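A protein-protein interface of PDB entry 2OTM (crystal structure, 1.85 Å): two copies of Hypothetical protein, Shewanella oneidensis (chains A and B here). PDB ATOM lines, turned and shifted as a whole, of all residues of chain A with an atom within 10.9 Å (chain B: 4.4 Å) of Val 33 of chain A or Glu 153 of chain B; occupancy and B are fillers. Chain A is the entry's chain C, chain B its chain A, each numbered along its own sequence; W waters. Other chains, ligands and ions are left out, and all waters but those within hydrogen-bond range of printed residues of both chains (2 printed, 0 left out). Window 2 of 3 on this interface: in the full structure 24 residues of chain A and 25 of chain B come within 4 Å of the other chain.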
ATOM      1  N   TYR A  30      15.036  -1.704  32.755  1.00  0.00           N
ATOM      2  CA  TYR A  30      13.662  -2.066  32.455  1.00  0.00           C
ATOM      3  C   TYR A  30      13.619  -2.858  31.178  1.00  0.00           C
ATOM      4  O   TYR A  30      14.597  -2.855  30.423  1.00  0.00           O
ATOM      5  CB  TYR A  30      12.800  -0.803  32.305  1.00  0.00           C
ATOM      6  CG  TYR A  30      13.208   0.114  31.163  1.00  0.00           C
ATOM      7  CD1 TYR A  30      12.697  -0.066  29.883  1.00  0.00           C
ATOM      8  CD2 TYR A  30      14.084   1.169  31.378  1.00  0.00           C
ATOM      9  CE1 TYR A  30      13.062   0.777  28.842  1.00  0.00           C
ATOM     10  CE2 TYR A  30      14.465   2.009  30.346  1.00  0.00           C
ATOM     11  CZ  TYR A  30      13.961   1.806  29.082  1.00  0.00           C
ATOM     12  OH  TYR A  30      14.323   2.651  28.055  1.00  0.00           O
ATOM     13  N   SER A  31      12.522  -3.574  30.957  1.00  0.00           N
ATOM     14  CA  SER A  31      12.300  -4.191  29.668  1.00  0.00           C
ATOM     15  C   SER A  31      10.841  -4.055  29.295  1.00  0.00           C
ATOM     16  O   SER A  31      10.013  -3.633  30.117  1.00  0.00           O
ATOM     17  CB  SER A  31      12.799  -5.630  29.635  1.00  0.00           C
ATOM     18  OG  SER A  31      12.119  -6.429  30.541  1.00  0.00           O
ATOM     19  N   ILE A  32      10.547  -4.347  28.030  1.00  0.00           N
ATOM     20  CA  ILE A  32       9.190  -4.173  27.477  1.00  0.00           C
ATOM     21  C   ILE A  32       8.861  -5.380  26.623  1.00  0.00           C
ATOM     22  O   ILE A  32       9.640  -5.750  25.752  1.00  0.00           O
ATOM     23  CB  ILE A  32       9.044  -2.883  26.591  1.00  0.00           C
ATOM     24  CG1 ILE A  32       9.492  -1.637  27.354  1.00  0.00           C
ATOM     25  CG2 ILE A  32       7.572  -2.674  26.078  1.00  0.00           C
ATOM     26  CD1 ILE A  32       9.467  -0.339  26.538  1.00  0.00           C
ATOM     27  N   VAL A  33       7.723  -6.008  26.895  1.00  0.00           N
ATOM     28  CA  VAL A  33       7.188  -7.034  26.018  1.00  0.00           C
ATOM     29  C   VAL A  33       5.752  -6.604  25.696  1.00  0.00           C
ATOM     30  O   VAL A  33       4.930  -6.379  26.580  1.00  0.00           O
ATOM     31  CB  VAL A  33       7.269  -8.443  26.590  1.00  0.00           C
ATOM     32  CG1 VAL A  33       6.476  -8.607  27.886  1.00  0.00           C
ATOM     33  CG2 VAL A  33       6.788  -9.436  25.511  1.00  0.00           C
ATOM     34  N   GLY A  34       5.480  -6.421  24.417  1.00  0.00           N
ATOM     35  CA  GLY A  34       4.211  -5.868  24.000  1.00  0.00           C
ATOM     36  C   GLY A  34       3.904  -4.545  24.674  1.00  0.00           C
ATOM     37  O   GLY A  34       4.619  -3.561  24.507  1.00  0.00           O
ATOM     38  N   SER A  35       2.823  -4.507  25.438  1.00  0.00           N
ATOM     39  CA  SER A  35       2.430  -3.273  26.111  1.00  0.00           C
ATOM     40  C   SER A  35       2.856  -3.264  27.581  1.00  0.00           C
ATOM     41  O   SER A  35       2.451  -2.388  28.330  1.00  0.00           O
ATOM     42  CB  SER A  35       0.925  -3.086  26.030  1.00  0.00           C
ATOM     43  OG  SER A  35       0.284  -4.045  26.840  1.00  0.00           O
ATOM     44  N   GLN A  36       3.690  -4.211  27.983  1.00  0.00           N
ATOM     45  CA  GLN A  36       4.040  -4.357  29.385  1.00  0.00           C
ATOM     46  C   GLN A  36       5.480  -3.928  29.606  1.00  0.00           C
ATOM     47  O   GLN A  36       6.403  -4.512  29.045  1.00  0.00           O
ATOM     48  CB  GLN A  36       3.836  -5.793  29.831  1.00  0.00           C
ATOM     49  CG  GLN A  36       2.363  -6.242  29.834  1.00  0.00           C
ATOM     50  CD  GLN A  36       2.198  -7.759  29.886  1.00  0.00           C
ATOM     51  OE1 GLN A  36       2.879  -8.451  30.624  1.00  0.00           O
ATOM     52  NE2 GLN A  36       1.292  -8.266  29.088  1.00  0.00           N
ATOM     53  N   LEU A  37       5.645  -2.919  30.454  1.00  0.00           N
ATOM     54  CA  LEU A  37       6.939  -2.354  30.836  1.00  0.00           C
ATOM     55  C   LEU A  37       7.226  -2.788  32.259  1.00  0.00           C
ATOM     56  O   LEU A  37       6.379  -2.642  33.106  1.00  0.00           O
ATOM     57  CB  LEU A  37       6.833  -0.820  30.768  1.00  0.00           C
ATOM     58  CG  LEU A  37       7.881   0.133  31.385  1.00  0.00           C
ATOM     59  CD1 LEU A  37       9.246  -0.087  30.775  1.00  0.00           C
ATOM     60  CD2 LEU A  37       7.423   1.609  31.238  1.00  0.00           C
ATOM     61  N   MET A  38       8.418  -3.318  32.518  1.00  0.00           N
ATOM     62  CA  MET A  38       8.742  -3.792  33.848  1.00  0.00           C
ATOM     63  C   MET A  38      10.132  -3.326  34.228  1.00  0.00           C
ATOM     64  O   MET A  38      11.066  -3.340  33.390  1.00  0.00           O
ATOM     65  CB  MET A  38       8.688  -5.307  33.853  1.00  0.00           C
ATOM     66  CG  MET A  38       9.592  -5.905  32.867  1.00  0.00           C
ATOM     67  SD  MET A  38       9.034  -7.732  32.582  1.00  0.00           S
ATOM     68  CE  MET A  38       7.335  -7.597  31.922  1.00  0.00           C
ATOM     69  N   THR A  39      10.271  -2.901  35.473  1.00  0.00           N
ATOM     70  CA  THR A  39      11.573  -2.488  36.007  1.00  0.00           C
ATOM     71  C   THR A  39      12.345  -3.661  36.609  1.00  0.00           C
ATOM     72  O   THR A  39      11.780  -4.688  36.925  1.00  0.00           O
ATOM     73  CB  THR A  39      11.439  -1.348  37.066  1.00  0.00           C
ATOM     74  OG1 THR A  39      11.024  -1.875  38.332  1.00  0.00           O
ATOM     75  CG2 THR A  39      10.464  -0.288  36.586  1.00  0.00           C
ATOM     76  N   ALA A  83      11.925   5.522  30.823  1.00  0.00           N
ATOM     77  CA  ALA A  83      11.481   4.615  29.779  1.00  0.00           C
ATOM     78  C   ALA A  83      10.376   5.169  28.890  1.00  0.00           C
ATOM     79  O   ALA A  83      10.376   4.894  27.697  1.00  0.00           O
ATOM     80  CB  ALA A  83      11.037   3.261  30.390  1.00  0.00           C
ATOM     81  N   TYR A  94      -0.072  -1.811  36.994  1.00  0.00           N
ATOM     82  CA  TYR A  94      -0.952  -2.924  37.348  1.00  0.00           C
ATOM     83  C   TYR A  94      -0.391  -3.841  38.435  1.00  0.00           C
ATOM     84  O   TYR A  94      -1.133  -4.599  39.047  1.00  0.00           O
ATOM     85  CB  TYR A  94      -1.342  -3.772  36.120  1.00  0.00           C
ATOM     86  CG  TYR A  94      -0.213  -4.448  35.360  1.00  0.00           C
ATOM     87  CD1 TYR A  94       0.411  -3.826  34.296  1.00  0.00           C
ATOM     88  CD2 TYR A  94       0.199  -5.729  35.676  1.00  0.00           C
ATOM     89  CE1 TYR A  94       1.429  -4.462  33.590  1.00  0.00           C
ATOM     90  CE2 TYR A  94       1.225  -6.342  34.993  1.00  0.00           C
ATOM     91  CZ  TYR A  94       1.819  -5.717  33.941  1.00  0.00           C
ATOM     92  OH  TYR A  94       2.833  -6.354  33.277  1.00  0.00           O
ATOM     93  N   LEU A 150       8.211  -2.464  39.634  1.00  0.00           N
ATOM     94  CA  LEU A 150       6.924  -2.013  39.097  1.00  0.00           C
ATOM     95  C   LEU A 150       6.691  -2.564  37.693  1.00  0.00           C
ATOM     96  O   LEU A 150       7.648  -2.816  36.941  1.00  0.00           O
ATOM     97  CB  LEU A 150       6.834  -0.467  39.053  1.00  0.00           C
ATOM     98  CG  LEU A 150       6.988   0.334  40.342  1.00  0.00           C
ATOM     99  CD1 LEU A 150       6.754   1.824  40.089  1.00  0.00           C
ATOM    100  CD2 LEU A 150       6.048  -0.210  41.405  1.00  0.00           C
ATOM    101  N   PHE A 151       5.414  -2.805  37.380  1.00  0.00           N
ATOM    102  CA  PHE A 151       4.963  -3.275  36.084  1.00  0.00           C
ATOM    103  C   PHE A 151       3.868  -2.331  35.615  1.00  0.00           C
ATOM    104  O   PHE A 151       2.898  -2.079  36.330  1.00  0.00           O
ATOM    105  CB  PHE A 151       4.394  -4.688  36.155  1.00  0.00           C
ATOM    106  CG  PHE A 151       5.343  -5.703  36.699  1.00  0.00           C
ATOM    107  CD1 PHE A 151       5.656  -5.738  38.063  1.00  0.00           C
ATOM    108  CD2 PHE A 151       5.875  -6.669  35.874  1.00  0.00           C
ATOM    109  CE1 PHE A 151       6.536  -6.672  38.566  1.00  0.00           C
ATOM    110  CE2 PHE A 151       6.755  -7.640  36.389  1.00  0.00           C
ATOM    111  CZ  PHE A 151       7.085  -7.626  37.733  1.00  0.00           C
ATOM    112  N   ALA A 152       4.032  -1.820  34.404  1.00  0.00           N
ATOM    113  CA  ALA A 152       3.165  -0.819  33.834  1.00  0.00           C
ATOM    114  C   ALA A 152       2.659  -1.267  32.475  1.00  0.00           C
ATOM    115  O   ALA A 152       3.394  -1.920  31.708  1.00  0.00           O
ATOM    116  CB  ALA A 152       3.945   0.479  33.647  1.00  0.00           C
ATOM    117  N   GLU A 153       1.425  -0.864  32.170  1.00  0.00           N
ATOM    118  CA  GLU A 153       0.830  -1.039  30.871  1.00  0.00           C
ATOM    119  C   GLU A 153       0.930   0.268  30.092  1.00  0.00           C
ATOM    120  O   GLU A 153       0.529   1.321  30.606  1.00  0.00           O
ATOM    121  CB  GLU A 153      -0.645  -1.367  31.013  1.00  0.00           C
ATOM    122  CG  GLU A 153      -1.249  -1.826  29.717  1.00  0.00           C
ATOM    123  CD  GLU A 153      -2.751  -1.995  29.770  1.00  0.00           C
ATOM    124  OE1 GLU A 153      -3.371  -1.706  30.818  1.00  0.00           O
ATOM    125  OE2 GLU A 153      -3.310  -2.414  28.736  1.00  0.00           O
ATOM    126  N   LEU A 154       1.447   0.197  28.874  1.00  0.00           N
ATOM    127  CA  LEU A 154       1.505   1.344  27.969  1.00  0.00           C
ATOM    128  C   LEU A 154       0.441   1.198  26.905  1.00  0.00           C
ATOM    129  O   LEU A 154      -0.207   0.159  26.824  1.00  0.00           O
ATOM    130  CB  LEU A 154       2.875   1.436  27.293  1.00  0.00           C
ATOM    131  CG  LEU A 154       4.091   1.588  28.201  1.00  0.00           C
ATOM    132  CD1 LEU A 154       5.359   1.473  27.389  1.00  0.00           C
ATOM    133  CD2 LEU A 154       4.052   2.876  28.970  1.00  0.00           C
ATOM    134  OXT LEU A 154       0.220   2.109  26.088  1.00  0.00           O
ATOM    135  N   SER B  35       2.274 -14.099  23.427  1.00  0.00           N
ATOM    136  CA  SER B  35       3.582 -14.179  22.833  1.00  0.00           C
ATOM    137  C   SER B  35       4.645 -14.366  23.910  1.00  0.00           C
ATOM    138  O   SER B  35       5.822 -14.214  23.630  1.00  0.00           O
ATOM    139  CB  SER B  35       3.812 -12.887  22.079  1.00  0.00           C
ATOM    140  OG  SER B  35       3.789 -11.796  22.991  1.00  0.00           O
ATOM    141  N   GLN B  36       4.215 -14.703  25.136  1.00  0.00           N
ATOM    142  CA  GLN B  36       5.096 -14.789  26.283  1.00  0.00           C
ATOM    143  C   GLN B  36       5.248 -16.216  26.761  1.00  0.00           C
ATOM    144  O   GLN B  36       4.275 -16.827  27.208  1.00  0.00           O
ATOM    145  CB  GLN B  36       4.536 -13.954  27.435  1.00  0.00           C
ATOM    146  CG  GLN B  36       4.631 -12.472  27.187  1.00  0.00           C
ATOM    147  CD  GLN B  36       3.734 -11.679  28.086  1.00  0.00           C
ATOM    148  OE1 GLN B  36       3.977 -11.570  29.289  1.00  0.00           O
ATOM    149  NE2 GLN B  36       2.672 -11.137  27.520  1.00  0.00           N
ATOM    150  N   ILE B  90      13.150 -16.711  18.908  1.00  0.00           N
ATOM    151  CA  ILE B  90      12.896 -15.908  20.109  1.00  0.00           C
ATOM    152  C   ILE B  90      13.236 -14.454  19.807  1.00  0.00           C
ATOM    153  O   ILE B  90      14.364 -14.130  19.413  1.00  0.00           O
ATOM    154  CB  ILE B  90      13.698 -16.445  21.291  1.00  0.00           C
ATOM    155  CG1 ILE B  90      13.194 -17.837  21.657  1.00  0.00           C
ATOM    156  CG2 ILE B  90      13.553 -15.529  22.500  1.00  0.00           C
ATOM    157  CD1 ILE B  90      14.142 -18.578  22.517  1.00  0.00           C
ATOM    158  N   LYS B  91      12.243 -13.591  19.969  1.00  0.00           N
ATOM    159  CA  LYS B  91      12.429 -12.150  19.714  1.00  0.00           C
ATOM    160  C   LYS B  91      13.276 -11.503  20.800  1.00  0.00           C
ATOM    161  O   LYS B  91      14.157 -10.683  20.519  1.00  0.00           O
ATOM    162  CB  LYS B  91      11.077 -11.465  19.604  1.00  0.00           C
ATOM    163  CG  LYS B  91      10.284 -11.966  18.442  1.00  0.00           C
ATOM    164  CD  LYS B  91       8.993 -11.236  18.282  1.00  0.00           C
ATOM    165  CE  LYS B  91       8.265 -11.741  17.047  1.00  0.00           C
ATOM    166  NZ  LYS B  91       6.939 -11.087  16.926  1.00  0.00           N
ATOM    167  N   GLN B  92      13.026 -11.886  22.047  1.00  0.00           N
ATOM    168  CA  GLN B  92      13.820 -11.401  23.162  1.00  0.00           C
ATOM    169  C   GLN B  92      13.642 -12.286  24.376  1.00  0.00           C
ATOM    170  O   GLN B  92      12.564 -12.847  24.590  1.00  0.00           O
ATOM    171  CB  GLN B  92      13.468  -9.963  23.541  1.00  0.00           C
ATOM    172  CG  GLN B  92      12.075  -9.753  24.041  1.00  0.00           C
ATOM    173  CD  GLN B  92      11.749  -8.299  24.462  1.00  0.00           C
ATOM    174  OE1 GLN B  92      12.609  -7.539  24.964  1.00  0.00           O
ATOM    175  NE2 GLN B  92      10.484  -7.927  24.282  1.00  0.00           N
ATOM    176  N   TYR B  94      13.331 -11.256  27.695  1.00  0.00           N
ATOM    177  CA  TYR B  94      13.103  -9.954  28.262  1.00  0.00           C
ATOM    178  C   TYR B  94      13.265  -9.901  29.767  1.00  0.00           C
ATOM    179  O   TYR B  94      13.407  -8.822  30.330  1.00  0.00           O
ATOM    180  CB  TYR B  94      11.725  -9.418  27.859  1.00  0.00           C
ATOM    181  CG  TYR B  94      10.531 -10.238  28.288  1.00  0.00           C
ATOM    182  CD1 TYR B  94       9.914 -10.027  29.521  1.00  0.00           C
ATOM    183  CD2 TYR B  94       9.987 -11.198  27.451  1.00  0.00           C
ATOM    184  CE1 TYR B  94       8.826 -10.751  29.913  1.00  0.00           C
ATOM    185  CE2 TYR B  94       8.908 -11.945  27.856  1.00  0.00           C
ATOM    186  CZ  TYR B  94       8.308 -11.697  29.078  1.00  0.00           C
ATOM    187  OH  TYR B  94       7.200 -12.421  29.476  1.00  0.00           O
ATOM    188  N   ALA B 152      10.539 -15.244  27.691  1.00  0.00           N
ATOM    189  CA  ALA B 152      10.891 -14.984  26.299  1.00  0.00           C
ATOM    190  C   ALA B 152       9.683 -14.507  25.527  1.00  0.00           C
ATOM    191  O   ALA B 152       8.557 -14.971  25.759  1.00  0.00           O
ATOM    192  CB  ALA B 152      11.430 -16.272  25.662  1.00  0.00           C
ATOM    193  N   GLU B 153       9.912 -13.583  24.602  1.00  0.00           N
ATOM    194  CA  GLU B 153       8.894 -13.166  23.670  1.00  0.00           C
ATOM    195  C   GLU B 153       9.036 -13.988  22.382  1.00  0.00           C
ATOM    196  O   GLU B 153      10.137 -14.086  21.830  1.00  0.00           O
ATOM    197  CB  GLU B 153       9.036 -11.684  23.341  1.00  0.00           C
ATOM    198  CG  GLU B 153       7.888 -11.157  22.534  1.00  0.00           C
ATOM    199  CD  GLU B 153       8.111  -9.717  22.095  1.00  0.00           C
ATOM    200  OE1 GLU B 153       9.202  -9.158  22.336  1.00  0.00           O
ATOM    201  OE2 GLU B 153       7.204  -9.147  21.493  1.00  0.00           O
ATOM    202  N   LEU B 154       7.911 -14.556  21.947  1.00  0.00           N
ATOM    203  CA  LEU B 154       7.812 -15.445  20.777  1.00  0.00           C
ATOM    204  C   LEU B 154       7.124 -14.729  19.615  1.00  0.00           C
ATOM    205  O   LEU B 154       7.197 -15.233  18.487  1.00  0.00           O
ATOM    206  CB  LEU B 154       6.926 -16.660  21.068  1.00  0.00           C
ATOM    207  CG  LEU B 154       7.138 -17.511  22.303  1.00  0.00           C
ATOM    208  CD1 LEU B 154       5.989 -18.537  22.452  1.00  0.00           C
ATOM    209  CD2 LEU B 154       8.498 -18.177  22.251  1.00  0.00           C
ATOM    210  OXT LEU B 154       6.443 -13.698  19.776  1.00  0.00           O
HETATM  211  O   HOH W   1       7.504  -6.416  22.295  1.00  0.00           O
HETATM  212  O   HOH W   2      12.769  -4.932  26.268  1.00  0.00           O
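The backbone carbonyl oxygen (O) of Ile 32 of chain A lies within hydrogen-bond range of the side-chain amide nitrogen (NE2) of Gln 92 of chain B, 2.8 Å away.
The side-chain hydroxyl of Ser 31 of chain A is in hydrogen-bond range of the backbone carbonyl oxygen of Tyr 94 of chain B (2.7 Å).
OE1 of Glu 153 of chain B sits at hydrogen-bond distance from NE2 of Gln 92 of chain B, at 2.6 Å.
N of Ser 31 of chain A sits at hydrogen-bond distance from O of Met 38 of chain A, at 2.8 Å.
The backbone NH of Lys 91 of chain B is in hydrogen-bond range of the backbone carbonyl oxygen of Glu 153 of chain B, at 2.9 Å.
The side-chain amide oxygen (OE1) of Gln 36 of chain B lies within hydrogen-bond range of the side-chain hydroxyl (OH) of Tyr 94 of chain B, at 3.3 Å.
OH of Tyr 94 of chain A lies within hydrogen-bond range of OE1 of Gln 36 of chain A, 3.4 Å away.
Among the printed residues, merely in contact across the chains: Gln 36 of chain A with Gln 36 of chain B, Val 33 of chain A with Glu 153 of chain B, Val 33 of chain A with Tyr 94 of chain B, Val 33 of chain A with Gln 92 of chain B and Met 38 of chain A with Tyr 94 of chain B.
Of chain B, only Gln 92 (3.8 Å), Tyr 94 (3.8 Å) and Glu 153 (3.6 Å) come within 4 Å of Val 33 of chain A.
Glu 153 of chain B touches just one residue of chain A: Val 33.
No residue of chain A comes within 4 Å of Ser 35 of chain B.
No residue of chain A comes within 4 Å of Lys 91 of chain B.
Gln 92 of chain B touches just these residues of chain A: Ile 32 and Val 33.
No residue of chain A comes within 4 Å of Leu 154 of chain B.
Printed residues of chain B within 4 Å of Gln 36 of chain A: Gln 36.
Of the printed residues of chain B, Met 38 of chain A touches Tyr 94 (3.9 Å).
Of the printed residues of chain B, Ile 32 of chain A touches Gln 92.
Printed residues of chain A within 4 Å of Gln 36 of chain B: Gln 36 (3.6 Å).
Tyr 30 of chain A touches none of the printed residues of chain B.
Ala 83 of chain A touches none of the printed residues of chain B.
Hydrophobic or aromatic side chains of chain B that line the printed part of chain A: Tyr 94.
Of the 17 printed residues of chain A, 5 touch a printed residue of chain B.
Among the printed residues, no Asp or Glu carboxylate lies within 4 Å of a Lys or Arg side-chain nitrogen of the other chain.
Gln 36 of chain A touches its own counterpart, Gln 36 of chain B.
Positions printed for both chains: 35, 36, 94, 152, 153 and 154.
Of the 7 pairs that touch across the chains among the printed residues, 1 has its exchanged pair printed and touching as well.
Water W1 lies within hydrogen-bond range of the side-chain carboxylate of Glu 153 of chain B and the backbone NH of Gly 34 of chain A.
Water W2 lies within hydrogen-bond range of the backbone NH of Ile 32 of chain A and the side-chain amide oxygen of Gln 92 of chain B.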
